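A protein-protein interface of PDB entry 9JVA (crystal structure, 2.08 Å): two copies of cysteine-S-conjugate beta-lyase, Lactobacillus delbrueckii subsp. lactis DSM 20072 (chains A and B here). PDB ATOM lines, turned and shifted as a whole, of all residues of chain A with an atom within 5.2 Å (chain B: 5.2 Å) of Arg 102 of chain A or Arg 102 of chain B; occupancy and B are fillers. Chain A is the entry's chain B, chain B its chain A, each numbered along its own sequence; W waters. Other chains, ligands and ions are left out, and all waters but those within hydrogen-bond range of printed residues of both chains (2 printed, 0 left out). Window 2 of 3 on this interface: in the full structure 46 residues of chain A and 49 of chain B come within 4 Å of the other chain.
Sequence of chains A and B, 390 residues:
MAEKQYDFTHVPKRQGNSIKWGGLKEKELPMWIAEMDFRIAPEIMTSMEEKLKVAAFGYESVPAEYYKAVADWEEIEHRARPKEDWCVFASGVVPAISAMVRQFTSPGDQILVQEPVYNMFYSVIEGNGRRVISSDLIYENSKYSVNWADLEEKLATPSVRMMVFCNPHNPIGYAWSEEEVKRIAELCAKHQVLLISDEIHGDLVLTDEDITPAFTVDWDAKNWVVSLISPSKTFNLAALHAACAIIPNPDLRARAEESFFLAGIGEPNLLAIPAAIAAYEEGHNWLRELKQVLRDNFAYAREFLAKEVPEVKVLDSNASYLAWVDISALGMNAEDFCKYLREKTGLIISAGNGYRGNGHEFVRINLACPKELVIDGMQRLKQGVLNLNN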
ATOM      1  N   ILE A  97     -14.137  10.222 -17.318  1.00  0.00           N
ATOM      2  CA  ILE A  97     -13.252   9.095 -17.602  1.00  0.00           C
ATOM      3  C   ILE A  97     -12.434   8.739 -16.365  1.00  0.00           C
ATOM      4  O   ILE A  97     -12.278   7.555 -16.015  1.00  0.00           O
ATOM      5  CB  ILE A  97     -12.348   9.411 -18.813  1.00  0.00           C
ATOM      6  CG1 ILE A  97     -13.181   9.534 -20.089  1.00  0.00           C
ATOM      7  CG2 ILE A  97     -11.304   8.323 -19.000  1.00  0.00           C
ATOM      8  CD1 ILE A  97     -12.382   9.968 -21.293  1.00  0.00           C
ATOM      9  N   SER A  98     -11.910   9.755 -15.669  1.00  0.00           N
ATOM     10  CA  SER A  98     -11.081   9.492 -14.496  1.00  0.00           C
ATOM     11  C   SER A  98     -11.857   8.722 -13.434  1.00  0.00           C
ATOM     12  O   SER A  98     -11.340   7.757 -12.856  1.00  0.00           O
ATOM     13  CB  SER A  98     -10.526  10.803 -13.931  1.00  0.00           C
ATOM     14  OG  SER A  98      -9.584  10.560 -12.895  1.00  0.00           O
ATOM     15  N   ALA A  99     -13.116   9.101 -13.206  1.00  0.00           N
ATOM     16  CA  ALA A  99     -13.952   8.420 -12.223  1.00  0.00           C
ATOM     17  C   ALA A  99     -14.243   6.979 -12.638  1.00  0.00           C
ATOM     18  O   ALA A  99     -14.209   6.069 -11.799  1.00  0.00           O
ATOM     19  CB  ALA A  99     -15.252   9.201 -12.018  1.00  0.00           C
ATOM     20  N   MET A 100     -14.526   6.747 -13.926  1.00  0.00           N
ATOM     21  CA  MET A 100     -14.797   5.390 -14.395  1.00  0.00           C
ATOM     22  C   MET A 100     -13.535   4.528 -14.411  1.00  0.00           C
ATOM     23  O   MET A 100     -13.624   3.310 -14.204  1.00  0.00           O
ATOM     24  CB  MET A 100     -15.456   5.444 -15.780  1.00  0.00           C
ATOM     25  CG  MET A 100     -16.848   6.066 -15.685  1.00  0.00           C
ATOM     26  SD  MET A 100     -17.811   6.123 -17.201  1.00  0.00           S
ATOM     27  CE  MET A 100     -16.711   7.140 -18.217  1.00  0.00           C
ATOM     28  N   VAL A 101     -12.359   5.133 -14.627  1.00  0.00           N
ATOM     29  CA  VAL A 101     -11.113   4.387 -14.442  1.00  0.00           C
ATOM     30  C   VAL A 101     -11.042   3.849 -13.017  1.00  0.00           C
ATOM     31  O   VAL A 101     -10.747   2.670 -12.786  1.00  0.00           O
ATOM     32  CB  VAL A 101      -9.898   5.273 -14.770  1.00  0.00           C
ATOM     33  CG1 VAL A 101      -8.600   4.604 -14.304  1.00  0.00           C
ATOM     34  CG2 VAL A 101      -9.812   5.540 -16.248  1.00  0.00           C
ATOM     35  N   ARG A 102     -11.340   4.702 -12.032  1.00  0.00           N
ATOM     36  CA  ARG A 102     -11.277   4.244 -10.650  1.00  0.00           C
ATOM     37  C   ARG A 102     -12.391   3.239 -10.337  1.00  0.00           C
ATOM     38  O   ARG A 102     -12.162   2.271  -9.605  1.00  0.00           O
ATOM     39  CB  ARG A 102     -11.327   5.438  -9.690  1.00  0.00           C
ATOM     40  CG  ARG A 102     -10.019   6.250  -9.643  1.00  0.00           C
ATOM     41  CD  ARG A 102      -9.998   7.259  -8.489  1.00  0.00           C
ATOM     42  NE  ARG A 102     -11.147   8.156  -8.566  1.00  0.00           N
ATOM     43  CZ  ARG A 102     -11.225   9.192  -9.395  1.00  0.00           C
ATOM     44  NH1 ARG A 102     -10.199   9.479 -10.191  1.00  0.00           N
ATOM     45  NH2 ARG A 102     -12.314   9.941  -9.422  1.00  0.00           N
ATOM     46  N   GLN A 103     -13.591   3.429 -10.889  1.00  0.00           N
ATOM     47  CA  GLN A 103     -14.709   2.570 -10.497  1.00  0.00           C
ATOM     48  C   GLN A 103     -14.672   1.211 -11.183  1.00  0.00           C
ATOM     49  O   GLN A 103     -15.088   0.200 -10.600  1.00  0.00           O
ATOM     50  CB  GLN A 103     -16.042   3.244 -10.817  1.00  0.00           C
ATOM     51  CG  GLN A 103     -17.164   2.698  -9.966  1.00  0.00           C
ATOM     52  CD  GLN A 103     -16.849   2.918  -8.509  1.00  0.00           C
ATOM     53  OE1 GLN A 103     -16.441   4.022  -8.116  1.00  0.00           O
ATOM     54  NE2 GLN A 103     -16.977   1.870  -7.705  1.00  0.00           N
ATOM     55  N   PHE A 104     -14.224   1.172 -12.432  1.00  0.00           N
ATOM     56  CA  PHE A 104     -14.446   0.015 -13.276  1.00  0.00           C
ATOM     57  C   PHE A 104     -13.173  -0.753 -13.577  1.00  0.00           C
ATOM     58  O   PHE A 104     -13.226  -1.746 -14.303  1.00  0.00           O
ATOM     59  CB  PHE A 104     -15.129   0.449 -14.580  1.00  0.00           C
ATOM     60  CG  PHE A 104     -16.476   1.087 -14.362  1.00  0.00           C
ATOM     61  CD1 PHE A 104     -17.333   0.596 -13.389  1.00  0.00           C
ATOM     62  CD2 PHE A 104     -16.881   2.153 -15.128  1.00  0.00           C
ATOM     63  CE1 PHE A 104     -18.582   1.177 -13.183  1.00  0.00           C
ATOM     64  CE2 PHE A 104     -18.130   2.741 -14.930  1.00  0.00           C
ATOM     65  CZ  PHE A 104     -18.972   2.257 -13.956  1.00  0.00           C
ATOM     66  N   THR A 105     -12.034  -0.313 -13.067  1.00  0.00           N
ATOM     67  CA  THR A 105     -10.801  -1.094 -13.154  1.00  0.00           C
ATOM     68  C   THR A 105     -10.130  -1.100 -11.790  1.00  0.00           C
ATOM     69  O   THR A 105     -10.504  -0.348 -10.892  1.00  0.00           O
ATOM     70  CB  THR A 105      -9.817  -0.530 -14.193  1.00  0.00           C
ATOM     71  OG1 THR A 105      -9.284   0.715 -13.716  1.00  0.00           O
ATOM     72  CG2 THR A 105     -10.489  -0.321 -15.564  1.00  0.00           C
ATOM     73  N   ASN A 128      -3.916   7.595 -12.244  1.00  0.00           N
ATOM     74  CA  ASN A 128      -4.755   6.778 -11.381  1.00  0.00           C
ATOM     75  C   ASN A 128      -4.129   5.442 -11.034  1.00  0.00           C
ATOM     76  O   ASN A 128      -4.787   4.609 -10.400  1.00  0.00           O
ATOM     77  CB  ASN A 128      -6.116   6.550 -12.044  1.00  0.00           C
ATOM     78  CG  ASN A 128      -7.082   7.689 -11.780  1.00  0.00           C
ATOM     79  OD1 ASN A 128      -7.318   8.048 -10.627  1.00  0.00           O
ATOM     80  ND2 ASN A 128      -7.613   8.290 -12.846  1.00  0.00           N
ATOM     81  N   ARG A 130      -3.248   3.084 -13.219  1.00  0.00           N
ATOM     82  CA  ARG A 130      -3.480   2.070 -14.231  1.00  0.00           C
ATOM     83  C   ARG A 130      -2.392   2.223 -15.291  1.00  0.00           C
ATOM     84  O   ARG A 130      -1.610   3.177 -15.269  1.00  0.00           O
ATOM     85  CB  ARG A 130      -4.895   2.180 -14.808  1.00  0.00           C
ATOM     86  CG  ARG A 130      -6.017   1.569 -13.908  1.00  0.00           C
ATOM     87  CD  ARG A 130      -6.184   2.256 -12.533  1.00  0.00           C
ATOM     88  NE  ARG A 130      -7.382   1.796 -11.810  1.00  0.00           N
ATOM     89  CZ  ARG A 130      -7.710   2.135 -10.556  1.00  0.00           C
ATOM     90  NH1 ARG A 130      -6.946   2.955  -9.837  1.00  0.00           N
ATOM     91  NH2 ARG A 130      -8.811   1.651 -10.006  1.00  0.00           N
ATOM     92  N   LEU A 262     -19.178  10.699  -5.783  1.00  0.00           N
ATOM     93  CA  LEU A 262     -18.092  10.546  -4.821  1.00  0.00           C
ATOM     94  C   LEU A 262     -16.871  11.372  -5.208  1.00  0.00           C
ATOM     95  O   LEU A 262     -16.169  11.883  -4.329  1.00  0.00           O
ATOM     96  CB  LEU A 262     -17.715   9.077  -4.694  1.00  0.00           C
ATOM     97  CG  LEU A 262     -16.769   8.736  -3.550  1.00  0.00           C
ATOM     98  CD1 LEU A 262     -17.454   8.974  -2.204  1.00  0.00           C
ATOM     99  CD2 LEU A 262     -16.289   7.287  -3.695  1.00  0.00           C
ATOM    100  N   ALA A 263     -16.607  11.528  -6.508  1.00  0.00           N
ATOM    101  CA  ALA A 263     -15.470  12.333  -6.938  1.00  0.00           C
ATOM    102  C   ALA A 263     -15.750  13.829  -6.888  1.00  0.00           C
ATOM    103  O   ALA A 263     -14.803  14.625  -6.907  1.00  0.00           O
ATOM    104  CB  ALA A 263     -15.044  11.943  -8.354  1.00  0.00           C
ATOM    105  N   ILE B  97     -11.871  16.840   0.106  1.00  0.00           N
ATOM    106  CA  ILE B  97     -11.717  15.834   1.152  1.00  0.00           C
ATOM    107  C   ILE B  97     -11.718  14.445   0.539  1.00  0.00           C
ATOM    108  O   ILE B  97     -10.903  13.583   0.903  1.00  0.00           O
ATOM    109  CB  ILE B  97     -12.818  15.972   2.219  1.00  0.00           C
ATOM    110  CG1 ILE B  97     -12.718  17.328   2.934  1.00  0.00           C
ATOM    111  CG2 ILE B  97     -12.705  14.838   3.228  1.00  0.00           C
ATOM    112  CD1 ILE B  97     -13.882  17.650   3.895  1.00  0.00           C
ATOM    113  N   SER B  98     -12.623  14.209  -0.415  1.00  0.00           N
ATOM    114  CA  SER B  98     -12.700  12.911  -1.071  1.00  0.00           C
ATOM    115  C   SER B  98     -11.390  12.579  -1.788  1.00  0.00           C
ATOM    116  O   SER B  98     -10.866  11.463  -1.669  1.00  0.00           O
ATOM    117  CB  SER B  98     -13.883  12.889  -2.041  1.00  0.00           C
ATOM    118  OG  SER B  98     -14.100  11.577  -2.523  1.00  0.00           O
ATOM    119  N   ALA B  99     -10.826  13.549  -2.511  1.00  0.00           N
ATOM    120  CA  ALA B  99      -9.550  13.312  -3.176  1.00  0.00           C
ATOM    121  C   ALA B  99      -8.444  12.999  -2.163  1.00  0.00           C
ATOM    122  O   ALA B  99      -7.627  12.091  -2.380  1.00  0.00           O
ATOM    123  CB  ALA B  99      -9.188  14.513  -4.058  1.00  0.00           C
ATOM    124  N   MET B 100      -8.428  13.701  -1.026  1.00  0.00           N
ATOM    125  CA  MET B 100      -7.354  13.510  -0.057  1.00  0.00           C
ATOM    126  C   MET B 100      -7.517  12.229   0.751  1.00  0.00           C
ATOM    127  O   MET B 100      -6.515  11.633   1.161  1.00  0.00           O
ATOM    128  CB  MET B 100      -7.268  14.724   0.869  1.00  0.00           C
ATOM    129  CG  MET B 100      -6.811  15.966   0.123  1.00  0.00           C
ATOM    130  SD  MET B 100      -6.449  17.354   1.196  1.00  0.00           S
ATOM    131  CE  MET B 100      -8.085  17.753   1.803  1.00  0.00           C
ATOM    132  N   VAL B 101      -8.758  11.794   0.990  1.00  0.00           N
ATOM    133  CA  VAL B 101      -8.985  10.455   1.534  1.00  0.00           C
ATOM    134  C   VAL B 101      -8.326   9.402   0.646  1.00  0.00           C
ATOM    135  O   VAL B 101      -7.617   8.504   1.125  1.00  0.00           O
ATOM    136  CB  VAL B 101     -10.492  10.194   1.693  1.00  0.00           C
ATOM    137  CG1 VAL B 101     -10.755   8.683   1.840  1.00  0.00           C
ATOM    138  CG2 VAL B 101     -11.041  10.965   2.885  1.00  0.00           C
ATOM    139  N   ARG B 102      -8.547   9.492  -0.667  1.00  0.00           N
ATOM    140  CA  ARG B 102      -7.970   8.487  -1.554  1.00  0.00           C
ATOM    141  C   ARG B 102      -6.451   8.602  -1.628  1.00  0.00           C
ATOM    142  O   ARG B 102      -5.765   7.591  -1.824  1.00  0.00           O
ATOM    143  CB  ARG B 102      -8.567   8.604  -2.955  1.00  0.00           C
ATOM    144  CG  ARG B 102     -10.017   8.163  -3.088  1.00  0.00           C
ATOM    145  CD  ARG B 102     -10.416   8.057  -4.571  1.00  0.00           C
ATOM    146  NE  ARG B 102     -10.307   9.343  -5.264  1.00  0.00           N
ATOM    147  CZ  ARG B 102     -11.206  10.319  -5.167  1.00  0.00           C
ATOM    148  NH1 ARG B 102     -12.306  10.149  -4.424  1.00  0.00           N
ATOM    149  NH2 ARG B 102     -11.021  11.452  -5.824  1.00  0.00           N
ATOM    150  N   GLN B 103      -5.908   9.810  -1.476  1.00  0.00           N
ATOM    151  CA  GLN B 103      -4.483  10.035  -1.687  1.00  0.00           C
ATOM    152  C   GLN B 103      -3.632   9.741  -0.458  1.00  0.00           C
ATOM    153  O   GLN B 103      -2.480   9.304  -0.601  1.00  0.00           O
ATOM    154  CB  GLN B 103      -4.239  11.486  -2.121  1.00  0.00           C
ATOM    155  CG  GLN B 103      -2.893  11.671  -2.773  1.00  0.00           C
ATOM    156  CD  GLN B 103      -2.775  10.870  -4.059  1.00  0.00           C
ATOM    157  OE1 GLN B 103      -3.663  10.907  -4.915  1.00  0.00           O
ATOM    158  NE2 GLN B 103      -1.695  10.114  -4.185  1.00  0.00           N
ATOM    159  N   PHE B 104      -4.173   9.962   0.738  1.00  0.00           N
ATOM    160  CA  PHE B 104      -3.396   9.992   1.970  1.00  0.00           C
ATOM    161  C   PHE B 104      -3.771   8.893   2.959  1.00  0.00           C
ATOM    162  O   PHE B 104      -3.217   8.856   4.065  1.00  0.00           O
ATOM    163  CB  PHE B 104      -3.551  11.365   2.637  1.00  0.00           C
ATOM    164  CG  PHE B 104      -3.056  12.497   1.789  1.00  0.00           C
ATOM    165  CD1 PHE B 104      -1.874  12.380   1.077  1.00  0.00           C
ATOM    166  CD2 PHE B 104      -3.767  13.677   1.698  1.00  0.00           C
ATOM    167  CE1 PHE B 104      -1.401  13.430   0.285  1.00  0.00           C
ATOM    168  CE2 PHE B 104      -3.305  14.721   0.921  1.00  0.00           C
ATOM    169  CZ  PHE B 104      -2.115  14.599   0.210  1.00  0.00           C
ATOM    170  N   THR B 105      -4.726   8.032   2.613  1.00  0.00           N
ATOM    171  CA  THR B 105      -5.054   6.843   3.393  1.00  0.00           C
ATOM    172  C   THR B 105      -5.200   5.655   2.453  1.00  0.00           C
ATOM    173  O   THR B 105      -5.221   5.798   1.225  1.00  0.00           O
ATOM    174  CB  THR B 105      -6.357   6.996   4.193  1.00  0.00           C
ATOM    175  OG1 THR B 105      -7.468   6.921   3.291  1.00  0.00           O
ATOM    176  CG2 THR B 105      -6.392   8.315   4.969  1.00  0.00           C
ATOM    177  N   ASN B 128     -15.555   5.868  -0.070  1.00  0.00           N
ATOM    178  CA  ASN B 128     -14.216   5.560  -0.552  1.00  0.00           C
ATOM    179  C   ASN B 128     -13.622   4.314   0.103  1.00  0.00           C
ATOM    180  O   ASN B 128     -12.460   3.992  -0.150  1.00  0.00           O
ATOM    181  CB  ASN B 128     -13.286   6.757  -0.322  1.00  0.00           C
ATOM    182  CG  ASN B 128     -13.466   7.841  -1.370  1.00  0.00           C
ATOM    183  OD1 ASN B 128     -13.185   7.633  -2.553  1.00  0.00           O
ATOM    184  ND2 ASN B 128     -13.958   8.998  -0.948  1.00  0.00           N
ATOM    185  N   ARG B 130     -13.006   3.666   3.348  1.00  0.00           N
ATOM    186  CA  ARG B 130     -12.328   3.862   4.612  1.00  0.00           C
ATOM    187  C   ARG B 130     -13.377   3.734   5.709  1.00  0.00           C
ATOM    188  O   ARG B 130     -14.584   3.719   5.444  1.00  0.00           O
ATOM    189  CB  ARG B 130     -11.601   5.218   4.628  1.00  0.00           C
ATOM    190  CG  ARG B 130     -10.233   5.210   3.893  1.00  0.00           C
ATOM    191  CD  ARG B 130     -10.328   4.928   2.384  1.00  0.00           C
ATOM    192  NE  ARG B 130      -9.087   5.239   1.659  1.00  0.00           N
ATOM    193  CZ  ARG B 130      -8.859   4.938   0.380  1.00  0.00           C
ATOM    194  NH1 ARG B 130      -9.766   4.294  -0.340  1.00  0.00           N
ATOM    195  NH2 ARG B 130      -7.709   5.267  -0.185  1.00  0.00           N
ATOM    196  N   LEU B 262      -6.336  14.977 -10.830  1.00  0.00           N
ATOM    197  CA  LEU B 262      -6.736  13.654 -11.291  1.00  0.00           C
ATOM    198  C   LEU B 262      -8.230  13.434 -11.120  1.00  0.00           C
ATOM    199  O   LEU B 262      -8.875  12.846 -11.993  1.00  0.00           O
ATOM    200  CB  LEU B 262      -5.931  12.582 -10.563  1.00  0.00           C
ATOM    201  CG  LEU B 262      -4.574  12.383 -11.250  1.00  0.00           C
ATOM    202  CD1 LEU B 262      -3.727  11.372 -10.512  1.00  0.00           C
ATOM    203  CD2 LEU B 262      -4.772  11.956 -12.699  1.00  0.00           C
ATOM    204  N   ALA B 263      -8.807  13.931 -10.022  1.00  0.00           N
ATOM    205  CA  ALA B 263     -10.240  13.813  -9.794  1.00  0.00           C
ATOM    206  C   ALA B 263     -11.075  14.731 -10.684  1.00  0.00           C
ATOM    207  O   ALA B 263     -12.299  14.564 -10.731  1.00  0.00           O
ATOM    208  CB  ALA B 263     -10.563  14.105  -8.330  1.00  0.00           C
HETATM  209  O   HOH W   1     -12.623  13.983  -5.308  1.00  0.00           O
HETATM  210  O   HOH W   2     -12.860  11.914 -11.426  1.00  0.00           O
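Among the printed residues, merely in contact across the chains: Leu 262 of chain A with Asn 128 of chain B (3.3 Å) and Arg 102 of chain A with Arg 102 of chain B (3.6 Å).
Of chain A, only Arg 102 (3.6 Å) comes within 4 Å of Arg 102 of chain B. Of the printed residues of chain B, Leu 262 of chain A touches Ser 98 (2.8 Å) and Asn 128 (3.3 Å). Of the printed residues of chain A, Leu 262 of chain B touches Ser 98 (2.6 Å). The nearest residue of chain B that does not touch Arg 102 of chain A is Leu 262 of chain B (4.04 Å). The nearest residue of chain A that does not touch Arg 102 of chain B is Leu 262 of chain A (4.2 Å). The nearest printed residue of chain B that does not touch Ser 98 of chain A is Ala 263 of chain B (4.5 Å).
Among the printed residues, 4 pairs touch across the chains. Among the printed residues, no Asp or Glu carboxylate lies within 4 Å of a Lys or Arg side-chain nitrogen of the other chain.
Water W1 lies within hydrogen-bond range of the backbone carbonyl oxygen of Ala 263 of chain A (2.8 Å), the guanidinium group of Arg 102 of chain B (3.0 Å) and the backbone NH of Ala 99 of chain B (3.4 Å). Water W2 lies within hydrogen-bond range of O of Ala 263 of chain B, NH2 of Arg 102 of chain A and N of Ala 99 of chain A.
The backbone carbonyl oxygen (O) of Arg 102 of chain B is in hydrogen-bond range of the guanidinium group (NH2) of Arg 130 of chain B, 3.4 Å away. NH1 of Arg 102 of chain B lies close to OD1 of Asn 128 of chain B, at 3.3 Å. OG of Ser 98 of chain B is in hydrogen-bond range of ND2 of Asn 128 of chain B (3.0 Å). The backbone carbonyl oxygen (O) of Arg 102 of chain A lies within hydrogen-bond range of the guanidinium group (NH2) of Arg 130 of chain A (3.4 Å). OG of Ser 98 of chain A is in hydrogen-bond range of NH1 of Arg 102 of chain A. The side-chain hydroxyl of Ser 98 of chain A is in hydrogen-bond range of the side-chain amide nitrogen of Asn 128 of chain A, at 3.0 Å.
O of Leu 262 of chain B lies within hydrogen-bond range of OG of Ser 98 of chain A. The backbone carbonyl oxygen of Leu 262 of chain A lies within hydrogen-bond range of the side-chain hydroxyl of Ser 98 of chain B (2.8 Å).
Ser 98 of chain A touches Leu 262 of chain B, and with the chains exchanged Leu 262 of chain A touches Ser 98 of chain B. Arg 102 of chain B touches its own counterpart, Arg 102 of chain A. Leu 262 of chain A touches Asn 128 of chain B, but with the chains exchanged Asn 128 of chain A does not touch Leu 262 of chain B (4.2 Å). Positions printed for both chains: 97, 98, 99, 100, 101, 102, 103, 104, 105, 128, 130, 262 and 263.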
